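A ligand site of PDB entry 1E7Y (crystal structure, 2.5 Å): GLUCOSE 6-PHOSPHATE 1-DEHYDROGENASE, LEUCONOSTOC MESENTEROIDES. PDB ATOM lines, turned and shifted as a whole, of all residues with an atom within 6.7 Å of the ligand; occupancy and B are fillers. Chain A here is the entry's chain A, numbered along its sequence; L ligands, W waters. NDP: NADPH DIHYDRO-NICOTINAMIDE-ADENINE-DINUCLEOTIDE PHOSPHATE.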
ATOM      1  N   PHE A  11      -6.458 -14.457   1.107  1.00  0.00           N
ATOM      2  CA  PHE A  11      -7.058 -13.140   0.955  1.00  0.00           C
ATOM      3  C   PHE A  11      -7.753 -13.185  -0.398  1.00  0.00           C
ATOM      4  O   PHE A  11      -7.108 -13.437  -1.426  1.00  0.00           O
ATOM      5  CB  PHE A  11      -5.996 -12.048   0.983  1.00  0.00           C
ATOM      6  CG  PHE A  11      -5.399 -11.829   2.350  1.00  0.00           C
ATOM      7  CD1 PHE A  11      -5.998 -10.960   3.250  1.00  0.00           C
ATOM      8  CD2 PHE A  11      -4.244 -12.499   2.735  1.00  0.00           C
ATOM      9  CE1 PHE A  11      -5.464 -10.751   4.512  1.00  0.00           C
ATOM     10  CE2 PHE A  11      -3.693 -12.304   4.000  1.00  0.00           C
ATOM     11  CZ  PHE A  11      -4.303 -11.430   4.888  1.00  0.00           C
ATOM     12  N   GLY A  12      -9.060 -12.953  -0.411  1.00  0.00           N
ATOM     13  CA  GLY A  12      -9.818 -13.013  -1.644  1.00  0.00           C
ATOM     14  C   GLY A  12     -10.300 -14.442  -1.780  1.00  0.00           C
ATOM     15  O   GLY A  12     -10.401 -14.984  -2.891  1.00  0.00           O
ATOM     16  N   GLY A  13     -10.620 -15.039  -0.633  1.00  0.00           N
ATOM     17  CA  GLY A  13     -11.072 -16.427  -0.577  1.00  0.00           C
ATOM     18  C   GLY A  13     -12.460 -16.745  -1.087  1.00  0.00           C
ATOM     19  O   GLY A  13     -12.935 -17.874  -0.928  1.00  0.00           O
ATOM     20  N   THR A  14     -13.143 -15.755  -1.651  1.00  0.00           N
ATOM     21  CA  THR A  14     -14.487 -15.954  -2.207  1.00  0.00           C
ATOM     22  C   THR A  14     -14.398 -15.752  -3.716  1.00  0.00           C
ATOM     23  O   THR A  14     -15.321 -16.110  -4.458  1.00  0.00           O
ATOM     24  CB  THR A  14     -15.518 -14.944  -1.611  1.00  0.00           C
ATOM     25  OG1 THR A  14     -15.003 -13.616  -1.669  1.00  0.00           O
ATOM     26  CG2 THR A  14     -15.841 -15.292  -0.164  1.00  0.00           C
ATOM     27  N   GLY A  15     -13.267 -15.204  -4.156  1.00  0.00           N
ATOM     28  CA  GLY A  15     -13.055 -14.930  -5.557  1.00  0.00           C
ATOM     29  C   GLY A  15     -13.050 -16.125  -6.485  1.00  0.00           C
ATOM     30  O   GLY A  15     -12.907 -17.275  -6.051  1.00  0.00           O
ATOM     31  N   ASP A  16     -13.162 -15.836  -7.772  1.00  0.00           N
ATOM     32  CA  ASP A  16     -13.187 -16.849  -8.816  1.00  0.00           C
ATOM     33  C   ASP A  16     -11.942 -17.741  -8.774  1.00  0.00           C
ATOM     34  O   ASP A  16     -12.060 -18.961  -8.810  1.00  0.00           O
ATOM     35  CB  ASP A  16     -13.316 -16.161 -10.183  1.00  0.00           C
ATOM     36  CG  ASP A  16     -13.395 -17.148 -11.348  1.00  0.00           C
ATOM     37  OD1 ASP A  16     -12.325 -17.507 -11.897  1.00  0.00           O
ATOM     38  OD2 ASP A  16     -14.523 -17.549 -11.724  1.00  0.00           O
ATOM     39  N   LEU A  17     -10.776 -17.128  -8.634  1.00  0.00           N
ATOM     40  CA  LEU A  17      -9.519 -17.881  -8.591  1.00  0.00           C
ATOM     41  C   LEU A  17      -9.459 -18.886  -7.460  1.00  0.00           C
ATOM     42  O   LEU A  17      -8.999 -20.013  -7.658  1.00  0.00           O
ATOM     43  CB  LEU A  17      -8.318 -16.943  -8.495  1.00  0.00           C
ATOM     44  CG  LEU A  17      -6.967 -17.678  -8.617  1.00  0.00           C
ATOM     45  CD1 LEU A  17      -6.734 -18.059 -10.065  1.00  0.00           C
ATOM     46  CD2 LEU A  17      -5.851 -16.791  -8.113  1.00  0.00           C
ATOM     47  N   ALA A  18      -9.863 -18.460  -6.265  1.00  0.00           N
ATOM     48  CA  ALA A  18      -9.844 -19.340  -5.114  1.00  0.00           C
ATOM     49  C   ALA A  18     -10.718 -20.559  -5.370  1.00  0.00           C
ATOM     50  O   ALA A  18     -10.347 -21.681  -5.054  1.00  0.00           O
ATOM     51  CB  ALA A  18     -10.324 -18.605  -3.884  1.00  0.00           C
ATOM     52  N   THR A  44     -10.651 -15.429   3.667  1.00  0.00           N
ATOM     53  CA  THR A  44     -10.999 -14.078   4.052  1.00  0.00           C
ATOM     54  C   THR A  44     -11.296 -13.187   2.860  1.00  0.00           C
ATOM     55  O   THR A  44     -10.693 -13.328   1.781  1.00  0.00           O
ATOM     56  CB  THR A  44      -9.912 -13.417   4.935  1.00  0.00           C
ATOM     57  OG1 THR A  44     -10.275 -12.075   5.256  1.00  0.00           O
ATOM     58  CG2 THR A  44      -8.563 -13.415   4.226  1.00  0.00           C
ATOM     59  N   ALA A  45     -12.242 -12.269   3.058  1.00  0.00           N
ATOM     60  CA  ALA A  45     -12.699 -11.305   2.075  1.00  0.00           C
ATOM     61  C   ALA A  45     -13.643 -10.393   2.854  1.00  0.00           C
ATOM     62  O   ALA A  45     -13.923 -10.661   4.028  1.00  0.00           O
ATOM     63  CB  ALA A  45     -13.451 -12.013   0.946  1.00  0.00           C
ATOM     64  N   ARG A  46     -14.113  -9.303   2.233  1.00  0.00           N
ATOM     65  CA  ARG A  46     -15.021  -8.366   2.897  1.00  0.00           C
ATOM     66  C   ARG A  46     -16.379  -9.004   3.178  1.00  0.00           C
ATOM     67  O   ARG A  46     -16.901  -8.912   4.300  1.00  0.00           O
ATOM     68  CB  ARG A  46     -15.249  -7.113   2.046  1.00  0.00           C
ATOM     69  CG  ARG A  46     -14.038  -6.267   1.822  1.00  0.00           C
ATOM     70  CD  ARG A  46     -14.411  -5.128   0.906  1.00  0.00           C
ATOM     71  NE  ARG A  46     -15.054  -5.620  -0.323  1.00  0.00           N
ATOM     72  CZ  ARG A  46     -15.235  -4.894  -1.422  1.00  0.00           C
ATOM     73  NH1 ARG A  46     -14.840  -3.633  -1.455  1.00  0.00           N
ATOM     74  NH2 ARG A  46     -15.800  -5.433  -2.486  1.00  0.00           N
ATOM     75  N   GLN A  47     -16.976  -9.580   2.136  1.00  0.00           N
ATOM     76  CA  GLN A  47     -18.272 -10.238   2.224  1.00  0.00           C
ATOM     77  C   GLN A  47     -18.368 -11.126   3.456  1.00  0.00           C
ATOM     78  O   GLN A  47     -17.433 -11.870   3.766  1.00  0.00           O
ATOM     79  CB  GLN A  47     -18.494 -11.074   0.970  1.00  0.00           C
ATOM     80  CG  GLN A  47     -19.785 -11.876   0.938  1.00  0.00           C
ATOM     81  CD  GLN A  47     -19.751 -12.994  -0.092  1.00  0.00           C
ATOM     82  OE1 GLN A  47     -20.577 -13.906  -0.046  1.00  0.00           O
ATOM     83  NE2 GLN A  47     -18.802 -12.933  -1.024  1.00  0.00           N
ATOM     84  N   ALA A  48     -19.478 -11.025   4.194  1.00  0.00           N
ATOM     85  CA  ALA A  48     -19.645 -11.825   5.398  1.00  0.00           C
ATOM     86  C   ALA A  48     -20.263 -13.168   5.070  1.00  0.00           C
ATOM     87  O   ALA A  48     -21.181 -13.249   4.264  1.00  0.00           O
ATOM     88  CB  ALA A  48     -20.513 -11.082   6.415  1.00  0.00           C
ATOM     89  N   TYR A  81     -13.444 -19.016   8.250  1.00  0.00           N
ATOM     90  CA  TYR A  81     -13.604 -17.771   7.522  1.00  0.00           C
ATOM     91  C   TYR A  81     -13.835 -16.615   8.488  1.00  0.00           C
ATOM     92  O   TYR A  81     -14.245 -16.835   9.631  1.00  0.00           O
ATOM     93  CB  TYR A  81     -14.806 -17.879   6.571  1.00  0.00           C
ATOM     94  CG  TYR A  81     -14.995 -16.710   5.620  1.00  0.00           C
ATOM     95  CD1 TYR A  81     -14.359 -16.684   4.384  1.00  0.00           C
ATOM     96  CD2 TYR A  81     -15.812 -15.627   5.953  1.00  0.00           C
ATOM     97  CE1 TYR A  81     -14.532 -15.626   3.500  1.00  0.00           C
ATOM     98  CE2 TYR A  81     -15.993 -14.552   5.069  1.00  0.00           C
ATOM     99  CZ  TYR A  81     -15.342 -14.562   3.843  1.00  0.00           C
ATOM    100  OH  TYR A  81     -15.506 -13.523   2.960  1.00  0.00           O
ATOM    101  N   HIS A  84     -13.659  -9.398   6.457  1.00  0.00           N
ATOM    102  CA  HIS A  84     -12.626  -8.423   6.778  1.00  0.00           C
ATOM    103  C   HIS A  84     -12.208  -7.512   5.628  1.00  0.00           C
ATOM    104  O   HIS A  84     -12.009  -7.968   4.506  1.00  0.00           O
ATOM    105  CB  HIS A  84     -11.405  -9.180   7.313  1.00  0.00           C
ATOM    106  CG  HIS A  84     -10.168  -8.346   7.419  1.00  0.00           C
ATOM    107  ND1 HIS A  84      -9.086  -8.508   6.580  1.00  0.00           N
ATOM    108  CD2 HIS A  84      -9.835  -7.346   8.265  1.00  0.00           C
ATOM    109  CE1 HIS A  84      -8.143  -7.653   6.908  1.00  0.00           C
ATOM    110  NE2 HIS A  84      -8.571  -6.932   7.923  1.00  0.00           N
ATOM    111  N   ASP A  85     -12.062  -6.228   5.917  1.00  0.00           N
ATOM    112  CA  ASP A  85     -11.630  -5.252   4.925  1.00  0.00           C
ATOM    113  C   ASP A  85     -10.130  -5.088   5.151  1.00  0.00           C
ATOM    114  O   ASP A  85      -9.689  -4.860   6.275  1.00  0.00           O
ATOM    115  CB  ASP A  85     -12.340  -3.912   5.131  1.00  0.00           C
ATOM    116  CG  ASP A  85     -12.022  -2.904   4.019  1.00  0.00           C
ATOM    117  OD1 ASP A  85     -11.767  -3.323   2.869  1.00  0.00           O
ATOM    118  OD2 ASP A  85     -12.067  -1.689   4.299  1.00  0.00           O
ATOM    119  N   VAL A  86      -9.358  -5.226   4.072  1.00  0.00           N
ATOM    120  CA  VAL A  86      -7.895  -5.115   4.165  1.00  0.00           C
ATOM    121  C   VAL A  86      -7.344  -3.737   4.514  1.00  0.00           C
ATOM    122  O   VAL A  86      -6.198  -3.623   4.977  1.00  0.00           O
ATOM    123  CB  VAL A  86      -7.216  -5.656   2.892  1.00  0.00           C
ATOM    124  CG1 VAL A  86      -7.454  -7.146   2.757  1.00  0.00           C
ATOM    125  CG2 VAL A  86      -7.737  -4.917   1.660  1.00  0.00           C
ATOM    126  N   THR A  87      -8.133  -2.700   4.290  1.00  0.00           N
ATOM    127  CA  THR A  87      -7.714  -1.331   4.594  1.00  0.00           C
ATOM    128  C   THR A  87      -8.037  -0.926   6.036  1.00  0.00           C
ATOM    129  O   THR A  87      -7.750   0.196   6.453  1.00  0.00           O
ATOM    130  CB  THR A  87      -8.375  -0.307   3.638  1.00  0.00           C
ATOM    131  OG1 THR A  87      -9.796  -0.483   3.651  1.00  0.00           O
ATOM    132  CG2 THR A  87      -7.878  -0.518   2.209  1.00  0.00           C
ATOM    133  N   SER A 117      -4.892 -13.292  -3.076  1.00  0.00           N
ATOM    134  CA  SER A 117      -5.711 -13.479  -4.268  1.00  0.00           C
ATOM    135  C   SER A 117      -6.667 -12.285  -4.330  1.00  0.00           C
ATOM    136  O   SER A 117      -7.892 -12.435  -4.341  1.00  0.00           O
ATOM    137  CB  SER A 117      -6.491 -14.799  -4.156  1.00  0.00           C
ATOM    138  OG  SER A 117      -7.182 -15.081  -5.360  1.00  0.00           O
ATOM    139  N   VAL A 118      -6.090 -11.081  -4.343  1.00  0.00           N
ATOM    140  CA  VAL A 118      -6.850  -9.837  -4.377  1.00  0.00           C
ATOM    141  C   VAL A 118      -6.222  -8.901  -5.405  1.00  0.00           C
ATOM    142  O   VAL A 118      -5.104  -9.146  -5.856  1.00  0.00           O
ATOM    143  CB  VAL A 118      -6.821  -9.100  -3.002  1.00  0.00           C
ATOM    144  CG1 VAL A 118      -7.486  -9.953  -1.934  1.00  0.00           C
ATOM    145  CG2 VAL A 118      -5.398  -8.780  -2.608  1.00  0.00           C
ATOM    146  N   ALA A 119      -6.935  -7.843  -5.767  1.00  0.00           N
ATOM    147  CA  ALA A 119      -6.426  -6.874  -6.735  1.00  0.00           C
ATOM    148  C   ALA A 119      -5.100  -6.298  -6.251  1.00  0.00           C
ATOM    149  O   ALA A 119      -4.905  -6.108  -5.053  1.00  0.00           O
ATOM    150  CB  ALA A 119      -7.453  -5.750  -6.937  1.00  0.00           C
ATOM    151  N   ARG A 121      -3.805  -3.350  -5.985  1.00  0.00           N
ATOM    152  CA  ARG A 121      -3.878  -2.167  -5.131  1.00  0.00           C
ATOM    153  C   ARG A 121      -3.851  -2.491  -3.628  1.00  0.00           C
ATOM    154  O   ARG A 121      -3.588  -1.614  -2.813  1.00  0.00           O
ATOM    155  CB  ARG A 121      -5.152  -1.374  -5.450  1.00  0.00           C
ATOM    156  CG  ARG A 121      -6.419  -2.181  -5.264  1.00  0.00           C
ATOM    157  CD  ARG A 121      -7.652  -1.462  -5.763  1.00  0.00           C
ATOM    158  NE  ARG A 121      -8.756  -2.401  -5.943  1.00  0.00           N
ATOM    159  CZ  ARG A 121      -9.802  -2.199  -6.734  1.00  0.00           C
ATOM    160  NH1 ARG A 121      -9.925  -1.068  -7.431  1.00  0.00           N
ATOM    161  NH2 ARG A 121     -10.729  -3.152  -6.862  1.00  0.00           N
ATOM    162  N   PHE A 122      -4.139  -3.737  -3.289  1.00  0.00           N
ATOM    163  CA  PHE A 122      -4.159  -4.175  -1.893  1.00  0.00           C
ATOM    164  C   PHE A 122      -2.895  -4.892  -1.439  1.00  0.00           C
ATOM    165  O   PHE A 122      -2.715  -5.096  -0.237  1.00  0.00           O
ATOM    166  CB  PHE A 122      -5.359  -5.082  -1.640  1.00  0.00           C
ATOM    167  CG  PHE A 122      -6.687  -4.448  -1.979  1.00  0.00           C
ATOM    168  CD1 PHE A 122      -7.025  -3.189  -1.485  1.00  0.00           C
ATOM    169  CD2 PHE A 122      -7.618  -5.121  -2.772  1.00  0.00           C
ATOM    170  CE1 PHE A 122      -8.260  -2.609  -1.769  1.00  0.00           C
ATOM    171  CE2 PHE A 122      -8.851  -4.563  -3.067  1.00  0.00           C
ATOM    172  CZ  PHE A 122      -9.180  -3.300  -2.572  1.00  0.00           C
ATOM    173  N   ILE A 126      -1.929  -4.925   2.628  1.00  0.00           N
ATOM    174  CA  ILE A 126      -2.041  -6.200   3.324  1.00  0.00           C
ATOM    175  C   ILE A 126      -0.722  -6.563   3.993  1.00  0.00           C
ATOM    176  O   ILE A 126      -0.698  -6.965   5.154  1.00  0.00           O
ATOM    177  CB  ILE A 126      -2.471  -7.304   2.372  1.00  0.00           C
ATOM    178  CG1 ILE A 126      -3.866  -6.995   1.808  1.00  0.00           C
ATOM    179  CG2 ILE A 126      -2.464  -8.644   3.076  1.00  0.00           C
ATOM    180  CD1 ILE A 126      -4.367  -7.991   0.789  1.00  0.00           C
HETATM  181  PA  NDP L   1     -12.832 -11.931  -8.001  1.00  0.00           P
HETATM  182  O1A NDP L   1     -14.299 -11.829  -7.919  1.00  0.00           O
HETATM  183  O2A NDP L   1     -12.371 -13.243  -8.527  1.00  0.00           O
HETATM  184  O5B NDP L   1     -12.316 -11.890  -6.488  1.00  0.00           O
HETATM  185  C5B NDP L   1     -12.067 -10.679  -5.777  1.00  0.00           C
HETATM  186  C4B NDP L   1     -11.700 -11.021  -4.345  1.00  0.00           C
HETATM  187  O4B NDP L   1     -11.153  -9.836  -3.703  1.00  0.00           O
HETATM  188  C3B NDP L   1     -12.983 -11.345  -3.592  1.00  0.00           C
HETATM  189  O3B NDP L   1     -12.789 -12.447  -2.707  1.00  0.00           O
HETATM  190  C2B NDP L   1     -13.232 -10.102  -2.788  1.00  0.00           C
HETATM  191  O2B NDP L   1     -13.898 -10.409  -1.575  1.00  0.00           O
HETATM  192  C1B NDP L   1     -11.835  -9.641  -2.482  1.00  0.00           C
HETATM  193  N9A NDP L   1     -11.799  -8.259  -1.952  1.00  0.00           N
HETATM  194  C8A NDP L   1     -12.043  -7.097  -2.629  1.00  0.00           C
HETATM  195  N7A NDP L   1     -11.751  -6.000  -1.968  1.00  0.00           N
HETATM  196  C5A NDP L   1     -11.372  -6.463  -0.745  1.00  0.00           C
HETATM  197  C6A NDP L   1     -10.988  -5.732   0.359  1.00  0.00           C
HETATM  198  N6A NDP L   1     -10.926  -4.378   0.198  1.00  0.00           N
HETATM  199  N1A NDP L   1     -10.682  -6.477   1.449  1.00  0.00           N
HETATM  200  C2A NDP L   1     -10.747  -7.804   1.407  1.00  0.00           C
HETATM  201  N3A NDP L   1     -11.045  -8.592   0.397  1.00  0.00           N
HETATM  202  C4A NDP L   1     -11.381  -7.839  -0.678  1.00  0.00           C
HETATM  203  O3  NDP L   1     -12.189 -10.780  -8.678  1.00  0.00           O
HETATM  204  P2B NDP L   1     -15.331  -9.755  -1.361  1.00  0.00           P
HETATM  205  O1X NDP L   1     -15.453  -8.676  -2.366  1.00  0.00           O
HETATM  206  O2X NDP L   1     -15.292  -9.224   0.014  1.00  0.00           O
HETATM  207  O3X NDP L   1     -16.315 -10.868  -1.498  1.00  0.00           O
HETATM  208  O   HOH W   1      -9.569  -9.713   3.993  1.00  0.00           O
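An oxygen (O2X) of the ligand sits at hydrogen-bond distance from the backbone NH of Arg 46 (2.5 Å).
The guanidinium group (NH2) of Arg 46 is in salt-bridge range of an oxygen (O1X) of the ligand, 3.3 Å away.
The backbone NH (N) of Thr 14 is in hydrogen-bond range of an oxygen (O3B) of the ligand (3.5 Å).
O3B of the ligand lies within hydrogen-bond range of OG1 of Thr 14, 2.7 Å away.
The backbone NH (N) of Gln 47 lies within hydrogen-bond range of an oxygen (O2X) of the ligand, at 2.7 Å.
NE2 of Gln 47 lies within hydrogen-bond range of O3X of the ligand, at 3.3 Å.
The backbone NH (N) of Asp 16 lies within hydrogen-bond range of an oxygen (O2A) of the ligand (2.8 Å).
The side-chain carboxylate of Asp 85 sits at hydrogen-bond distance from a nitrogen (N6A) of the ligand, at 3.0 Å.
An oxygen (O3B) of the ligand is in hydrogen-bond range of the backbone NH (N) of Gly 15 (3.2 Å).
A nitrogen (N1A) of the ligand sits at hydrogen-bond distance from the backbone NH of Val 86 (3.2 Å).
The backbone carbonyl oxygen (O) of Gly 12 lies close to an oxygen (O3B) of the ligand, at 3.5 Å.
The backbone carbonyl oxygen of His 84 sits at hydrogen-bond distance from the backbone NH of Arg 46 (3.4 Å).
O of Gln 47 sits at hydrogen-bond distance from OH of Tyr 81.
OD2 of Asp 85 sits at hydrogen-bond distance from OG1 of Thr 87 (2.7 Å).
The backbone carbonyl oxygen (O) of Ala 45 lies within hydrogen-bond range of the backbone NH (N) of His 84 (2.8 Å).
OH of Tyr 81 lies close to O of Ala 45.
The backbone carbonyl oxygen (O) of Thr 44 lies within hydrogen-bond range of the backbone NH (N) of Gly 12 (2.8 Å).
N of Gly 13 is in hydrogen-bond range of O of Thr 44 (3.0 Å).
Gly 13 touches the ligand.
CB of Ala 45 touches O2B of the ligand (3.0 Å).
His 84 touches the ligand.
CE2 of Phe 122 touches N7A of the ligand (3.4 Å).
Water W1 lies within hydrogen-bond range of the side-chain hydroxyl of Thr 44 (2.8 Å) and a ring nitrogen (ND1) of His 84 (2.9 Å).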
